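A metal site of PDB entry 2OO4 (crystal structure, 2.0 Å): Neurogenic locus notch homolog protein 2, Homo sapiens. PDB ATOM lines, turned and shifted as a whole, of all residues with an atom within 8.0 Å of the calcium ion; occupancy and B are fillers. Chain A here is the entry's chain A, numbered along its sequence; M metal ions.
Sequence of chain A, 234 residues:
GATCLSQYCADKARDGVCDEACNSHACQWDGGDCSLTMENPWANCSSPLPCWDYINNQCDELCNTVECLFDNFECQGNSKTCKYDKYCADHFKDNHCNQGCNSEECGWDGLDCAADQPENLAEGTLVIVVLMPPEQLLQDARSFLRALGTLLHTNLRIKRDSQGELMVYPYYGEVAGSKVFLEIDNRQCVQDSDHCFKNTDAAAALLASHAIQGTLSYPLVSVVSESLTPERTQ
The calcium ion is bound by the side-chain carboxylate (OE1) of Glu 74 (2.3 Å), the backbone carbonyl oxygen (O) of Tyr 54 (2.3 Å), the backbone carbonyl oxygen (O) of Gln 58 (2.4 Å), the side-chain carboxylate (OD2) of Asp 71 (2.4 Å), the side-chain carboxylate (OD1) of Asp 71 (2.6 Å), the side-chain amide oxygen (OD1) of Asn 56 (2.6 Å) and the side-chain carboxylate (OD2) of Asp 60 (2.7 Å).
N of Asp 60 lies within hydrogen-bond range of SG of Cys 75 (3.6 Å).
N of Cys 59 sits close to O of Glu 74 (3.4 Å).
N of Asp 71 sits at hydrogen-bond distance from O of Cys 63, 2.8 Å away.
OE2 of Glu 74 lies within hydrogen-bond range of N of Asn 57, at 2.8 Å.
The side-chain sulfur (SG) of Cys 51 forms a disulfide with the side-chain sulfur (SG) of Cys 63 (2.0 Å).
The side-chain sulfur of Cys 59 forms a disulfide with the side-chain sulfur of Cys 75, 2.0 Å away.
Six residues have an atom within 4 Å of the calcium ion: Tyr 54, Asn 56, Gln 58, Asp 60, Asp 71 and Glu 74.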
ATOM      1  N   LEU A  49       4.897 -23.042  27.078  1.00  0.00           N
ATOM      2  CA  LEU A  49       5.846 -21.932  27.043  1.00  0.00           C
ATOM      3  C   LEU A  49       6.577 -21.776  28.380  1.00  0.00           C
ATOM      4  O   LEU A  49       6.009 -22.039  29.435  1.00  0.00           O
ATOM      5  CB  LEU A  49       5.141 -20.614  26.700  1.00  0.00           C
ATOM      6  CG  LEU A  49       4.449 -20.409  25.346  1.00  0.00           C
ATOM      7  CD1 LEU A  49       3.887 -19.000  25.292  1.00  0.00           C
ATOM      8  CD2 LEU A  49       5.390 -20.653  24.152  1.00  0.00           C
ATOM      9  N   CYS A  51       6.922 -19.444  30.665  1.00  0.00           N
ATOM     10  CA  CYS A  51       6.152 -18.217  30.845  1.00  0.00           C
ATOM     11  C   CYS A  51       6.939 -17.040  31.440  1.00  0.00           C
ATOM     12  O   CYS A  51       6.583 -15.888  31.210  1.00  0.00           O
ATOM     13  CB  CYS A  51       4.875 -18.500  31.650  1.00  0.00           C
ATOM     14  SG  CYS A  51       3.632 -19.458  30.713  1.00  0.00           S
ATOM     15  N   ASP A  53       9.712 -16.111  30.394  1.00  0.00           N
ATOM     16  CA  ASP A  53      10.303 -15.444  29.237  1.00  0.00           C
ATOM     17  C   ASP A  53       9.299 -14.585  28.457  1.00  0.00           C
ATOM     18  O   ASP A  53       9.671 -13.828  27.564  1.00  0.00           O
ATOM     19  CB  ASP A  53      10.982 -16.455  28.310  1.00  0.00           C
ATOM     20  CG  ASP A  53      12.368 -16.856  28.789  1.00  0.00           C
ATOM     21  OD1 ASP A  53      12.961 -16.104  29.603  1.00  0.00           O
ATOM     22  OD2 ASP A  53      12.870 -17.913  28.339  1.00  0.00           O
ATOM     23  N   TYR A  54       8.018 -14.701  28.829  1.00  0.00           N
ATOM     24  CA  TYR A  54       6.947 -14.034  28.101  1.00  0.00           C
ATOM     25  C   TYR A  54       6.308 -12.850  28.821  1.00  0.00           C
ATOM     26  O   TYR A  54       5.195 -12.433  28.490  1.00  0.00           O
ATOM     27  CB  TYR A  54       5.896 -15.063  27.638  1.00  0.00           C
ATOM     28  CG  TYR A  54       6.399 -15.949  26.507  1.00  0.00           C
ATOM     29  CD1 TYR A  54       7.260 -17.026  26.768  1.00  0.00           C
ATOM     30  CD2 TYR A  54       6.033 -15.703  25.187  1.00  0.00           C
ATOM     31  CE1 TYR A  54       7.735 -17.828  25.746  1.00  0.00           C
ATOM     32  CE2 TYR A  54       6.496 -16.502  24.158  1.00  0.00           C
ATOM     33  CZ  TYR A  54       7.353 -17.566  24.434  1.00  0.00           C
ATOM     34  OH  TYR A  54       7.815 -18.365  23.405  1.00  0.00           O
ATOM     35  N   ILE A  55       7.024 -12.286  29.795  1.00  0.00           N
ATOM     36  CA  ILE A  55       6.685 -10.996  30.390  1.00  0.00           C
ATOM     37  C   ILE A  55       7.206  -9.919  29.425  1.00  0.00           C
ATOM     38  O   ILE A  55       8.342  -9.439  29.536  1.00  0.00           O
ATOM     39  CB  ILE A  55       7.294 -10.820  31.808  1.00  0.00           C
ATOM     40  CG1 ILE A  55       6.848 -11.959  32.726  1.00  0.00           C
ATOM     41  CG2 ILE A  55       6.913  -9.471  32.420  1.00  0.00           C
ATOM     42  CD1 ILE A  55       7.829 -12.297  33.821  1.00  0.00           C
ATOM     43  N   ASN A  56       6.354  -9.547  28.462  1.00  0.00           N
ATOM     44  CA  ASN A  56       6.788  -8.800  27.285  1.00  0.00           C
ATOM     45  C   ASN A  56       5.827  -7.692  26.843  1.00  0.00           C
ATOM     46  O   ASN A  56       5.958  -7.163  25.738  1.00  0.00           O
ATOM     47  CB  ASN A  56       7.036  -9.776  26.115  1.00  0.00           C
ATOM     48  CG  ASN A  56       5.874 -10.750  25.898  1.00  0.00           C
ATOM     49  OD1 ASN A  56       4.767 -10.521  26.360  1.00  0.00           O
ATOM     50  ND2 ASN A  56       6.140 -11.844  25.191  1.00  0.00           N
ATOM     51  N   ASN A  57       4.870  -7.357  27.708  1.00  0.00           N
ATOM     52  CA  ASN A  57       3.823  -6.354  27.429  1.00  0.00           C
ATOM     53  C   ASN A  57       2.932  -6.739  26.232  1.00  0.00           C
ATOM     54  O   ASN A  57       2.356  -5.881  25.553  1.00  0.00           O
ATOM     55  CB  ASN A  57       4.441  -4.951  27.257  1.00  0.00           C
ATOM     56  CG  ASN A  57       3.435  -3.834  27.490  1.00  0.00           C
ATOM     57  OD1 ASN A  57       3.089  -3.094  26.574  1.00  0.00           O
ATOM     58  ND2 ASN A  57       2.957  -3.719  28.731  1.00  0.00           N
ATOM     59  N   GLN A  58       2.805  -8.047  26.003  1.00  0.00           N
ATOM     60  CA  GLN A  58       1.987  -8.598  24.933  1.00  0.00           C
ATOM     61  C   GLN A  58       1.268  -9.855  25.424  1.00  0.00           C
ATOM     62  O   GLN A  58       1.846 -10.655  26.161  1.00  0.00           O
ATOM     63  CB  GLN A  58       2.847  -8.915  23.725  1.00  0.00           C
ATOM     64  N   CYS A  59       0.011 -10.013  25.022  1.00  0.00           N
ATOM     65  CA  CYS A  59      -0.787 -11.169  25.468  1.00  0.00           C
ATOM     66  C   CYS A  59      -0.309 -12.492  24.876  1.00  0.00           C
ATOM     67  O   CYS A  59      -0.278 -12.663  23.645  1.00  0.00           O
ATOM     68  CB  CYS A  59      -2.279 -10.966  25.198  1.00  0.00           C
ATOM     69  SG  CYS A  59      -3.317 -12.402  25.613  1.00  0.00           S
ATOM     70  N   ASP A  60       0.068 -13.407  25.750  1.00  0.00           N
ATOM     71  CA  ASP A  60       0.366 -14.781  25.380  1.00  0.00           C
ATOM     72  C   ASP A  60      -0.622 -15.693  26.087  1.00  0.00           C
ATOM     73  O   ASP A  60      -0.552 -15.891  27.303  1.00  0.00           O
ATOM     74  CB  ASP A  60       1.817 -15.131  25.739  1.00  0.00           C
ATOM     75  CG  ASP A  60       2.829 -14.320  24.937  1.00  0.00           C
ATOM     76  OD1 ASP A  60       2.965 -14.574  23.715  1.00  0.00           O
ATOM     77  OD2 ASP A  60       3.493 -13.451  25.533  1.00  0.00           O
ATOM     78  N   GLU A  61      -1.564 -16.241  25.318  1.00  0.00           N
ATOM     79  CA  GLU A  61      -2.682 -17.006  25.870  1.00  0.00           C
ATOM     80  C   GLU A  61      -2.252 -18.314  26.532  1.00  0.00           C
ATOM     81  O   GLU A  61      -2.914 -18.794  27.462  1.00  0.00           O
ATOM     82  CB  GLU A  61      -3.734 -17.295  24.786  1.00  0.00           C
ATOM     83  CG  GLU A  61      -4.653 -16.116  24.473  1.00  0.00           C
ATOM     84  CD  GLU A  61      -5.522 -15.688  25.664  1.00  0.00           C
ATOM     85  OE1 GLU A  61      -5.846 -14.492  25.746  1.00  0.00           O
ATOM     86  OE2 GLU A  61      -5.879 -16.544  26.511  1.00  0.00           O
ATOM     87  N   CYS A  63       0.085 -18.634  28.424  1.00  0.00           N
ATOM     88  CA  CYS A  63       0.462 -18.261  29.791  1.00  0.00           C
ATOM     89  C   CYS A  63      -0.663 -17.554  30.567  1.00  0.00           C
ATOM     90  O   CYS A  63      -0.478 -17.189  31.719  1.00  0.00           O
ATOM     91  CB  CYS A  63       1.712 -17.365  29.749  1.00  0.00           C
ATOM     92  SG  CYS A  63       3.170 -18.222  29.165  1.00  0.00           S
ATOM     93  N   ASN A  64      -1.818 -17.388  29.939  1.00  0.00           N
ATOM     94  CA  ASN A  64      -2.939 -16.698  30.579  1.00  0.00           C
ATOM     95  C   ASN A  64      -3.805 -17.646  31.423  1.00  0.00           C
ATOM     96  O   ASN A  64      -5.002 -17.848  31.145  1.00  0.00           O
ATOM     97  CB  ASN A  64      -3.758 -15.920  29.543  1.00  0.00           C
ATOM     98  CG  ASN A  64      -4.803 -14.998  30.167  1.00  0.00           C
ATOM     99  OD1 ASN A  64      -4.696 -14.594  31.330  1.00  0.00           O
ATOM    100  ND2 ASN A  64      -5.817 -14.670  29.399  1.00  0.00           N
ATOM    101  N   PHE A  70      -1.364 -15.614  35.020  1.00  0.00           N
ATOM    102  CA  PHE A  70      -2.190 -14.842  34.084  1.00  0.00           C
ATOM    103  C   PHE A  70      -1.326 -14.039  33.108  1.00  0.00           C
ATOM    104  O   PHE A  70      -1.676 -12.909  32.735  1.00  0.00           O
ATOM    105  CB  PHE A  70      -3.147 -13.894  34.833  1.00  0.00           C
ATOM    106  CG  PHE A  70      -4.167 -14.591  35.710  1.00  0.00           C
ATOM    107  CD1 PHE A  70      -4.149 -14.401  37.103  1.00  0.00           C
ATOM    108  CD2 PHE A  70      -5.165 -15.387  35.168  1.00  0.00           C
ATOM    109  CE1 PHE A  70      -5.101 -15.026  37.924  1.00  0.00           C
ATOM    110  CE2 PHE A  70      -6.116 -16.012  35.989  1.00  0.00           C
ATOM    111  CZ  PHE A  70      -6.087 -15.825  37.360  1.00  0.00           C
ATOM    112  N   ASP A  71      -0.191 -14.608  32.719  1.00  0.00           N
ATOM    113  CA  ASP A  71       0.766 -13.912  31.865  1.00  0.00           C
ATOM    114  C   ASP A  71       0.975 -12.465  32.364  1.00  0.00           C
ATOM    115  O   ASP A  71       0.895 -11.514  31.589  1.00  0.00           O
ATOM    116  CB  ASP A  71       0.285 -13.942  30.412  1.00  0.00           C
ATOM    117  CG  ASP A  71       1.308 -13.405  29.431  1.00  0.00           C
ATOM    118  OD1 ASP A  71       2.524 -13.673  29.594  1.00  0.00           O
ATOM    119  OD2 ASP A  71       0.903 -12.708  28.480  1.00  0.00           O
ATOM    120  N   ASN A  72       1.220 -12.318  33.671  1.00  0.00           N
ATOM    121  CA  ASN A  72       1.529 -10.997  34.256  1.00  0.00           C
ATOM    122  C   ASN A  72       0.453  -9.944  33.979  1.00  0.00           C
ATOM    123  O   ASN A  72       0.752  -8.743  33.902  1.00  0.00           O
ATOM    124  CB  ASN A  72       2.886 -10.509  33.731  1.00  0.00           C
ATOM    125  CG  ASN A  72       3.569  -9.558  34.697  1.00  0.00           C
ATOM    126  OD1 ASN A  72       3.818  -9.900  35.847  1.00  0.00           O
ATOM    127  ND2 ASN A  72       3.871  -8.354  34.223  1.00  0.00           N
ATOM    128  N   PHE A  73      -0.784 -10.413  33.814  1.00  0.00           N
ATOM    129  CA  PHE A  73      -1.923  -9.573  33.405  1.00  0.00           C
ATOM    130  C   PHE A  73      -1.714  -8.827  32.092  1.00  0.00           C
ATOM    131  O   PHE A  73      -2.189  -7.697  31.914  1.00  0.00           O
ATOM    132  CB  PHE A  73      -2.339  -8.604  34.530  1.00  0.00           C
ATOM    133  CG  PHE A  73      -2.817  -9.286  35.774  1.00  0.00           C
ATOM    134  CD1 PHE A  73      -2.226  -9.011  37.005  1.00  0.00           C
ATOM    135  CD2 PHE A  73      -3.854 -10.214  35.732  1.00  0.00           C
ATOM    136  CE1 PHE A  73      -2.675  -9.627  38.173  1.00  0.00           C
ATOM    137  CE2 PHE A  73      -4.287 -10.847  36.906  1.00  0.00           C
ATOM    138  CZ  PHE A  73      -3.703 -10.552  38.116  1.00  0.00           C
ATOM    139  N   GLU A  74      -1.003  -9.457  31.154  1.00  0.00           N
ATOM    140  CA  GLU A  74      -0.758  -8.871  29.828  1.00  0.00           C
ATOM    141  C   GLU A  74      -1.850  -9.222  28.800  1.00  0.00           C
ATOM    142  O   GLU A  74      -1.762  -8.841  27.634  1.00  0.00           O
ATOM    143  CB  GLU A  74       0.631  -9.267  29.310  1.00  0.00           C
ATOM    144  CG  GLU A  74       1.776  -8.747  30.179  1.00  0.00           C
ATOM    145  CD  GLU A  74       3.156  -9.116  29.662  1.00  0.00           C
ATOM    146  OE1 GLU A  74       3.263  -9.957  28.741  1.00  0.00           O
ATOM    147  OE2 GLU A  74       4.142  -8.556  30.175  1.00  0.00           O
ATOM    148  N   CYS A  75      -2.881  -9.936  29.266  1.00  0.00           N
ATOM    149  CA  CYS A  75      -4.010 -10.323  28.422  1.00  0.00           C
ATOM    150  C   CYS A  75      -5.292  -9.583  28.821  1.00  0.00           C
ATOM    151  O   CYS A  75      -6.400 -10.138  28.770  1.00  0.00           O
ATOM    152  CB  CYS A  75      -4.207 -11.839  28.451  1.00  0.00           C
ATOM    153  SG  CYS A  75      -2.923 -12.785  27.579  1.00  0.00           S
HETATM  154 CA    CA M   1       3.074 -11.954  27.721  1.00  0.00          CA
